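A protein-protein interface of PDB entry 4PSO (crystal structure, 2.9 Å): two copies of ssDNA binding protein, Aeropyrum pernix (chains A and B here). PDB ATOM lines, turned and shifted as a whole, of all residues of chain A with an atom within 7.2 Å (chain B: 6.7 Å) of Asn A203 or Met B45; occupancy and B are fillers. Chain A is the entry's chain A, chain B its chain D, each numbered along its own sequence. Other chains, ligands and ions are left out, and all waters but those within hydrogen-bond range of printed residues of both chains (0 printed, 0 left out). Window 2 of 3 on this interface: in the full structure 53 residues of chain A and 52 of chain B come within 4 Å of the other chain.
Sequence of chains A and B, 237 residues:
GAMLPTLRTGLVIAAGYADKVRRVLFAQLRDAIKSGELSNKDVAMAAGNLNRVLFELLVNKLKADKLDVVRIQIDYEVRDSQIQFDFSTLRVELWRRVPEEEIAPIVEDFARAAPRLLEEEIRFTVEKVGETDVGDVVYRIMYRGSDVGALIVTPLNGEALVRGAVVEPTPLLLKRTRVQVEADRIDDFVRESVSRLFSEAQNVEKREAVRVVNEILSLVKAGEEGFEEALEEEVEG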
ATOM      1  N   LEU A 118       8.568   5.592 -10.202  1.00  0.00           N
ATOM      2  CA  LEU A 118       9.414   4.753  -9.364  1.00  0.00           C
ATOM      3  C   LEU A 118       9.087   3.266  -9.482  1.00  0.00           C
ATOM      4  O   LEU A 118       9.942   2.416  -9.231  1.00  0.00           O
ATOM      5  CB  LEU A 118       9.294   5.219  -7.913  1.00  0.00           C
ATOM      6  CG  LEU A 118      10.324   4.767  -6.880  1.00  0.00           C
ATOM      7  CD1 LEU A 118      10.583   5.906  -5.901  1.00  0.00           C
ATOM      8  CD2 LEU A 118       9.857   3.519  -6.143  1.00  0.00           C
ATOM      9  N   ILE A 122      12.670   0.096 -15.873  1.00  0.00           N
ATOM     10  CA  ILE A 122      13.581   0.910 -16.668  1.00  0.00           C
ATOM     11  C   ILE A 122      13.939   0.317 -18.037  1.00  0.00           C
ATOM     12  O   ILE A 122      14.872  -0.480 -18.137  1.00  0.00           O
ATOM     13  CB  ILE A 122      14.890   1.171 -15.903  1.00  0.00           C
ATOM     14  CG1 ILE A 122      14.598   1.588 -14.459  1.00  0.00           C
ATOM     15  CG2 ILE A 122      15.706   2.232 -16.614  1.00  0.00           C
ATOM     16  CD1 ILE A 122      15.844   1.858 -13.645  1.00  0.00           C
ATOM     17  N   THR A 170      20.141   4.995 -13.058  1.00  0.00           N
ATOM     18  CA  THR A 170      20.683   4.710 -11.735  1.00  0.00           C
ATOM     19  C   THR A 170      21.689   3.564 -11.857  1.00  0.00           C
ATOM     20  O   THR A 170      21.481   2.638 -12.644  1.00  0.00           O
ATOM     21  CB  THR A 170      19.558   4.369 -10.722  1.00  0.00           C
ATOM     22  OG1 THR A 170      20.115   4.172  -9.416  1.00  0.00           O
ATOM     23  CG2 THR A 170      18.800   3.120 -11.151  1.00  0.00           C
ATOM     24  N   PRO A 171      22.804   3.645 -11.105  1.00  0.00           N
ATOM     25  CA  PRO A 171      23.868   2.636 -11.193  1.00  0.00           C
ATOM     26  C   PRO A 171      23.388   1.241 -10.813  1.00  0.00           C
ATOM     27  O   PRO A 171      23.016   1.003  -9.664  1.00  0.00           O
ATOM     28  CB  PRO A 171      24.919   3.141 -10.199  1.00  0.00           C
ATOM     29  CG  PRO A 171      24.669   4.610 -10.103  1.00  0.00           C
ATOM     30  CD  PRO A 171      23.181   4.764 -10.225  1.00  0.00           C
ATOM     31  N   LEU A 172      23.409   0.329 -11.777  1.00  0.00           N
ATOM     32  CA  LEU A 172      22.958  -1.035 -11.547  1.00  0.00           C
ATOM     33  C   LEU A 172      24.021  -2.047 -11.942  1.00  0.00           C
ATOM     34  O   LEU A 172      24.757  -1.852 -12.911  1.00  0.00           O
ATOM     35  CB  LEU A 172      21.665  -1.310 -12.322  1.00  0.00           C
ATOM     36  CG  LEU A 172      20.428  -0.496 -11.935  1.00  0.00           C
ATOM     37  CD1 LEU A 172      19.257  -0.766 -12.876  1.00  0.00           C
ATOM     38  CD2 LEU A 172      20.050  -0.834 -10.508  1.00  0.00           C
ATOM     39  N   LEU A 173      24.095  -3.131 -11.181  1.00  0.00           N
ATOM     40  CA  LEU A 173      25.016  -4.214 -11.487  1.00  0.00           C
ATOM     41  C   LEU A 173      24.248  -5.506 -11.703  1.00  0.00           C
ATOM     42  O   LEU A 173      23.548  -5.989 -10.809  1.00  0.00           O
ATOM     43  CB  LEU A 173      26.046  -4.397 -10.370  1.00  0.00           C
ATOM     44  CG  LEU A 173      27.074  -5.497 -10.645  1.00  0.00           C
ATOM     45  CD1 LEU A 173      27.949  -5.109 -11.824  1.00  0.00           C
ATOM     46  CD2 LEU A 173      27.925  -5.778  -9.415  1.00  0.00           C
ATOM     47  N   GLU A 200      15.896  -6.786 -11.799  1.00  0.00           N
ATOM     48  CA  GLU A 200      16.270  -7.541 -10.612  1.00  0.00           C
ATOM     49  C   GLU A 200      17.755  -7.342 -10.314  1.00  0.00           C
ATOM     50  O   GLU A 200      18.360  -8.105  -9.561  1.00  0.00           O
ATOM     51  CB  GLU A 200      15.941  -9.022 -10.805  1.00  0.00           C
ATOM     52  CG  GLU A 200      14.452  -9.288 -11.014  1.00  0.00           C
ATOM     53  CD  GLU A 200      14.143 -10.744 -11.315  1.00  0.00           C
ATOM     54  OE1 GLU A 200      15.093 -11.528 -11.526  1.00  0.00           O
ATOM     55  OE2 GLU A 200      12.947 -11.105 -11.348  1.00  0.00           O
ATOM     56  N   ALA A 201      18.332  -6.302 -10.908  1.00  0.00           N
ATOM     57  CA  ALA A 201      19.754  -6.012 -10.764  1.00  0.00           C
ATOM     58  C   ALA A 201      20.060  -5.327  -9.434  1.00  0.00           C
ATOM     59  O   ALA A 201      19.154  -4.837  -8.752  1.00  0.00           O
ATOM     60  CB  ALA A 201      20.227  -5.149 -11.922  1.00  0.00           C
ATOM     61  N   GLN A 202      21.339  -5.285  -9.072  1.00  0.00           N
ATOM     62  CA  GLN A 202      21.758  -4.654  -7.822  1.00  0.00           C
ATOM     63  C   GLN A 202      21.950  -3.151  -7.936  1.00  0.00           C
ATOM     64  O   GLN A 202      22.561  -2.665  -8.886  1.00  0.00           O
ATOM     65  CB  GLN A 202      23.067  -5.265  -7.318  1.00  0.00           C
ATOM     66  CG  GLN A 202      22.970  -6.686  -6.815  1.00  0.00           C
ATOM     67  CD  GLN A 202      24.212  -7.091  -6.050  1.00  0.00           C
ATOM     68  OE1 GLN A 202      25.330  -6.761  -6.447  1.00  0.00           O
ATOM     69  NE2 GLN A 202      24.023  -7.796  -4.938  1.00  0.00           N
ATOM     70  N   ASN A 203      21.448  -2.423  -6.945  1.00  0.00           N
ATOM     71  CA  ASN A 203      21.724  -0.999  -6.846  1.00  0.00           C
ATOM     72  C   ASN A 203      23.101  -0.776  -6.223  1.00  0.00           C
ATOM     73  O   ASN A 203      23.323  -1.109  -5.055  1.00  0.00           O
ATOM     74  CB  ASN A 203      20.643  -0.291  -6.031  1.00  0.00           C
ATOM     75  CG  ASN A 203      19.268  -0.403  -6.666  1.00  0.00           C
ATOM     76  OD1 ASN A 203      18.476  -1.282  -6.317  1.00  0.00           O
ATOM     77  ND2 ASN A 203      18.985   0.477  -7.622  1.00  0.00           N
ATOM     78  N   VAL A 204      24.028  -0.231  -7.007  1.00  0.00           N
ATOM     79  CA  VAL A 204      25.402  -0.047  -6.548  1.00  0.00           C
ATOM     80  C   VAL A 204      25.835   1.402  -6.698  1.00  0.00           C
ATOM     81  O   VAL A 204      25.040   2.258  -7.093  1.00  0.00           O
ATOM     82  CB  VAL A 204      26.393  -0.936  -7.330  1.00  0.00           C
ATOM     83  CG1 VAL A 204      26.079  -2.401  -7.106  1.00  0.00           C
ATOM     84  CG2 VAL A 204      26.342  -0.600  -8.814  1.00  0.00           C
ATOM     85  N   GLU A 205      27.101   1.668  -6.387  1.00  0.00           N
ATOM     86  CA  GLU A 205      27.676   2.998  -6.563  1.00  0.00           C
ATOM     87  C   GLU A 205      28.039   3.221  -8.027  1.00  0.00           C
ATOM     88  O   GLU A 205      28.250   2.262  -8.773  1.00  0.00           O
ATOM     89  CB  GLU A 205      28.907   3.176  -5.671  1.00  0.00           C
ATOM     90  CG  GLU A 205      28.580   3.245  -4.185  1.00  0.00           C
ATOM     91  CD  GLU A 205      29.716   3.809  -3.356  1.00  0.00           C
ATOM     92  OE1 GLU A 205      30.857   3.865  -3.861  1.00  0.00           O
ATOM     93  OE2 GLU A 205      29.464   4.194  -2.194  1.00  0.00           O
ATOM     94  N   GLU A 208      31.457   1.811  -9.421  1.00  0.00           N
ATOM     95  CA  GLU A 208      31.447   0.368  -9.601  1.00  0.00           C
ATOM     96  C   GLU A 208      30.850   0.031 -10.953  1.00  0.00           C
ATOM     97  O   GLU A 208      31.383  -0.792 -11.694  1.00  0.00           O
ATOM     98  CB  GLU A 208      30.647  -0.313  -8.499  1.00  0.00           C
ATOM     99  CG  GLU A 208      31.219  -0.133  -7.117  1.00  0.00           C
ATOM    100  CD  GLU A 208      30.478  -0.954  -6.093  1.00  0.00           C
ATOM    101  OE1 GLU A 208      29.773  -0.365  -5.247  1.00  0.00           O
ATOM    102  OE2 GLU A 208      30.605  -2.197  -6.129  1.00  0.00           O
ATOM    103  N   ARG B  22      23.476   7.938  -2.010  1.00  0.00           N
ATOM    104  CA  ARG B  22      23.542   6.564  -1.541  1.00  0.00           C
ATOM    105  C   ARG B  22      24.333   6.476  -0.231  1.00  0.00           C
ATOM    106  O   ARG B  22      23.915   5.803   0.714  1.00  0.00           O
ATOM    107  CB  ARG B  22      24.167   5.668  -2.618  1.00  0.00           C
ATOM    108  CG  ARG B  22      23.903   4.172  -2.436  1.00  0.00           C
ATOM    109  CD  ARG B  22      24.554   3.333  -3.537  1.00  0.00           C
ATOM    110  NE  ARG B  22      24.514   1.902  -3.237  1.00  0.00           N
ATOM    111  CZ  ARG B  22      25.439   1.249  -2.547  1.00  0.00           C
ATOM    112  NH1 ARG B  22      26.481   1.899  -2.052  1.00  0.00           N
ATOM    113  NH2 ARG B  22      25.313  -0.054  -2.338  1.00  0.00           N
ATOM    114  N   PHE B  26      22.913   5.582   3.588  1.00  0.00           N
ATOM    115  CA  PHE B  26      23.473   4.436   4.295  1.00  0.00           C
ATOM    116  C   PHE B  26      23.987   4.837   5.675  1.00  0.00           C
ATOM    117  O   PHE B  26      23.878   4.070   6.631  1.00  0.00           O
ATOM    118  CB  PHE B  26      24.598   3.795   3.480  1.00  0.00           C
ATOM    119  CG  PHE B  26      24.161   2.610   2.657  1.00  0.00           C
ATOM    120  CD1 PHE B  26      23.928   1.379   3.259  1.00  0.00           C
ATOM    121  CD2 PHE B  26      23.990   2.722   1.283  1.00  0.00           C
ATOM    122  CE1 PHE B  26      23.532   0.281   2.505  1.00  0.00           C
ATOM    123  CE2 PHE B  26      23.593   1.630   0.522  1.00  0.00           C
ATOM    124  CZ  PHE B  26      23.364   0.407   1.135  1.00  0.00           C
ATOM    125  N   ASN B  40      20.640  -4.239   3.879  1.00  0.00           N
ATOM    126  CA  ASN B  40      21.450  -3.436   2.973  1.00  0.00           C
ATOM    127  C   ASN B  40      20.772  -3.307   1.613  1.00  0.00           C
ATOM    128  O   ASN B  40      20.878  -2.272   0.949  1.00  0.00           O
ATOM    129  CB  ASN B  40      22.842  -4.041   2.811  1.00  0.00           C
ATOM    130  CG  ASN B  40      23.662  -3.959   4.079  1.00  0.00           C
ATOM    131  OD1 ASN B  40      24.239  -2.918   4.389  1.00  0.00           O
ATOM    132  ND2 ASN B  40      23.724  -5.061   4.816  1.00  0.00           N
ATOM    133  N   LYS B  41      20.057  -4.355   1.209  1.00  0.00           N
ATOM    134  CA  LYS B  41      19.340  -4.334  -0.056  1.00  0.00           C
ATOM    135  C   LYS B  41      18.223  -3.296  -0.024  1.00  0.00           C
ATOM    136  O   LYS B  41      18.025  -2.575  -0.997  1.00  0.00           O
ATOM    137  CB  LYS B  41      18.768  -5.716  -0.391  1.00  0.00           C
ATOM    138  CG  LYS B  41      18.106  -5.778  -1.763  1.00  0.00           C
ATOM    139  CD  LYS B  41      17.625  -7.177  -2.111  1.00  0.00           C
ATOM    140  CE  LYS B  41      17.031  -7.210  -3.515  1.00  0.00           C
ATOM    141  NZ  LYS B  41      16.634  -8.580  -3.955  1.00  0.00           N
ATOM    142  N   ASP B  42      17.510  -3.210   1.099  1.00  0.00           N
ATOM    143  CA  ASP B  42      16.406  -2.261   1.231  1.00  0.00           C
ATOM    144  C   ASP B  42      16.881  -0.822   1.067  1.00  0.00           C
ATOM    145  O   ASP B  42      16.228  -0.017   0.400  1.00  0.00           O
ATOM    146  CB  ASP B  42      15.709  -2.411   2.587  1.00  0.00           C
ATOM    147  CG  ASP B  42      14.891  -3.683   2.694  1.00  0.00           C
ATOM    148  OD1 ASP B  42      14.275  -4.091   1.687  1.00  0.00           O
ATOM    149  OD2 ASP B  42      14.854  -4.266   3.798  1.00  0.00           O
ATOM    150  N   VAL B  43      18.022  -0.507   1.674  1.00  0.00           N
ATOM    151  CA  VAL B  43      18.562   0.845   1.625  1.00  0.00           C
ATOM    152  C   VAL B  43      19.113   1.187   0.246  1.00  0.00           C
ATOM    153  O   VAL B  43      18.844   2.264  -0.284  1.00  0.00           O
ATOM    154  CB  VAL B  43      19.671   1.037   2.683  1.00  0.00           C
ATOM    155  CG1 VAL B  43      20.328   2.401   2.546  1.00  0.00           C
ATOM    156  CG2 VAL B  43      19.101   0.845   4.081  1.00  0.00           C
ATOM    157  N   ALA B  44      19.861   0.262  -0.342  1.00  0.00           N
ATOM    158  CA  ALA B  44      20.442   0.491  -1.656  1.00  0.00           C
ATOM    159  C   ALA B  44      19.346   0.642  -2.705  1.00  0.00           C
ATOM    160  O   ALA B  44      19.438   1.475  -3.611  1.00  0.00           O
ATOM    161  CB  ALA B  44      21.378  -0.635  -2.019  1.00  0.00           C
ATOM    162  N   MET B  45      18.308  -0.177  -2.563  1.00  0.00           N
ATOM    163  CA  MET B  45      17.149  -0.154  -3.443  1.00  0.00           C
ATOM    164  C   MET B  45      16.379   1.147  -3.275  1.00  0.00           C
ATOM    165  O   MET B  45      15.860   1.706  -4.242  1.00  0.00           O
ATOM    166  CB  MET B  45      16.259  -1.364  -3.143  1.00  0.00           C
ATOM    167  CG  MET B  45      16.122  -2.363  -4.277  1.00  0.00           C
ATOM    168  SD  MET B  45      15.191  -3.819  -3.753  1.00  0.00           S
ATOM    169  CE  MET B  45      13.844  -3.061  -2.843  1.00  0.00           C
ATOM    170  N   ALA B  46      16.322   1.634  -2.040  1.00  0.00           N
ATOM    171  CA  ALA B  46      15.619   2.875  -1.747  1.00  0.00           C
ATOM    172  C   ALA B  46      16.333   4.056  -2.385  1.00  0.00           C
ATOM    173  O   ALA B  46      15.703   4.916  -3.002  1.00  0.00           O
ATOM    174  CB  ALA B  46      15.495   3.073  -0.248  1.00  0.00           C
ATOM    175  N   ALA B  47      17.651   4.090  -2.217  1.00  0.00           N
ATOM    176  CA  ALA B  47      18.487   5.143  -2.780  1.00  0.00           C
ATOM    177  C   ALA B  47      18.505   5.093  -4.304  1.00  0.00           C
ATOM    178  O   ALA B  47      18.553   6.130  -4.966  1.00  0.00           O
ATOM    179  CB  ALA B  47      19.897   5.038  -2.233  1.00  0.00           C
ATOM    180  N   GLY B  48      18.484   3.880  -4.850  1.00  0.00           N
ATOM    181  CA  GLY B  48      18.500   3.686  -6.290  1.00  0.00           C
ATOM    182  C   GLY B  48      17.239   4.238  -6.922  1.00  0.00           C
ATOM    183  O   GLY B  48      17.278   4.851  -7.991  1.00  0.00           O
ATOM    184  N   ASN B  49      16.113   4.020  -6.251  1.00  0.00           N
ATOM    185  CA  ASN B  49      14.842   4.533  -6.731  1.00  0.00           C
ATOM    186  C   ASN B  49      14.815   6.053  -6.673  1.00  0.00           C
ATOM    187  O   ASN B  49      14.278   6.702  -7.571  1.00  0.00           O
ATOM    188  CB  ASN B  49      13.684   3.963  -5.912  1.00  0.00           C
ATOM    189  CG  ASN B  49      13.405   2.506  -6.225  1.00  0.00           C
ATOM    190  OD1 ASN B  49      13.674   2.029  -7.330  1.00  0.00           O
ATOM    191  ND2 ASN B  49      12.852   1.791  -5.251  1.00  0.00           N
ATOM    192  N   LEU B  50      15.410   6.615  -5.622  1.00  0.00           N
ATOM    193  CA  LEU B  50      15.500   8.065  -5.476  1.00  0.00           C
ATOM    194  C   LEU B  50      16.392   8.650  -6.561  1.00  0.00           C
ATOM    195  O   LEU B  50      16.048   9.655  -7.182  1.00  0.00           O
ATOM    196  CB  LEU B  50      16.038   8.442  -4.093  1.00  0.00           C
ATOM    197  CG  LEU B  50      16.217   9.938  -3.806  1.00  0.00           C
ATOM    198  CD1 LEU B  50      14.891  10.680  -3.928  1.00  0.00           C
ATOM    199  CD2 LEU B  50      16.816  10.153  -2.429  1.00  0.00           C
ATOM    200  N   PHE B  85       9.892   7.658   0.930  1.00  0.00           N
ATOM    201  CA  PHE B  85      10.192   9.069   0.718  1.00  0.00           C
ATOM    202  C   PHE B  85       8.916   9.903   0.634  1.00  0.00           C
ATOM    203  O   PHE B  85       7.914   9.458   0.071  1.00  0.00           O
ATOM    204  CB  PHE B  85      11.011   9.259  -0.561  1.00  0.00           C
ATOM    205  CG  PHE B  85      12.355   8.593  -0.527  1.00  0.00           C
ATOM    206  CD1 PHE B  85      13.423   9.190   0.127  1.00  0.00           C
ATOM    207  CD2 PHE B  85      12.554   7.373  -1.159  1.00  0.00           C
ATOM    208  CE1 PHE B  85      14.665   8.578   0.157  1.00  0.00           C
ATOM    209  CE2 PHE B  85      13.793   6.755  -1.134  1.00  0.00           C
ATOM    210  CZ  PHE B  85      14.850   7.359  -0.476  1.00  0.00           C
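The backbone carbonyl oxygen (O) of Pro A171 sits at hydrogen-bond distance from the backbone NH (N) of Val A204 (3.1 Å).
The backbone carbonyl oxygen of Met B45 is in hydrogen-bond range of the side-chain amide nitrogen of Asn B49 (3.2 Å).
CD2 of Leu A118 touches ND2 of Asn B49 (3.6 Å).
O of Asn A203 touches NH2 of Arg B22, 3.5 Å away.
CB of Asn A203 touches O of Ala B44, at 3.2 Å.
Met B45 touches Asn A203.
Asn A203 touches Gly B48 (ND2 to CA, 3.5 Å).
Val A204 touches Arg B22.
The side-chain hydroxyl (OG1) of Thr A170 lies within hydrogen-bond range of the backbone carbonyl oxygen (O) of Gly B48, 3.2 Å away.
The side-chain carboxylate (OE2) of Glu A205 lies within salt-bridge range of the guanidinium group (NH1) of Arg B22, at 3.8 Å.
No position is printed for both chains.
Of the 8 pairs that touch across the chains among the printed residues, none has its exchanged pair printed and touching as well.
Of chain B, only Arg B22 (3.5 Å), Ala B44 (3.2 Å), Met B45 (3.3 Å) and Gly B48 (3.5 Å) come within 4 Å of Asn A203.
Printed residues of chain A within 4 Å of Met B45: Asn A203 (3.3 Å).
Printed residues of chain A within 4 Å of Gly B48: Thr A170 and Asn A203.
Of the printed residues of chain B, Val A204 touches Arg B22.
Printed residues of chain A within 4 Å of Ala B44: Asn A203 (3.2 Å).
Val B43 touches none of the printed residues of chain A.
Gln A202 touches none of the printed residues of chain B.
The nearest residue of chain B that does not touch Asn A203 is Asn B49 (4.8 Å).
The nearest residue of chain A that does not touch Met B45 is Ala A201 (5.9 Å).
Hydrophobic or aromatic side chains of chain A within 4 Å of the printed part of chain B: Leu A118.
Hydrophobic or aromatic side chains of chain B within 4 Å of the printed part of chain A: Ala B44 and Met B45.
Along chain B the printed residues that touch a printed residue of chain A span positions 22 to 49.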
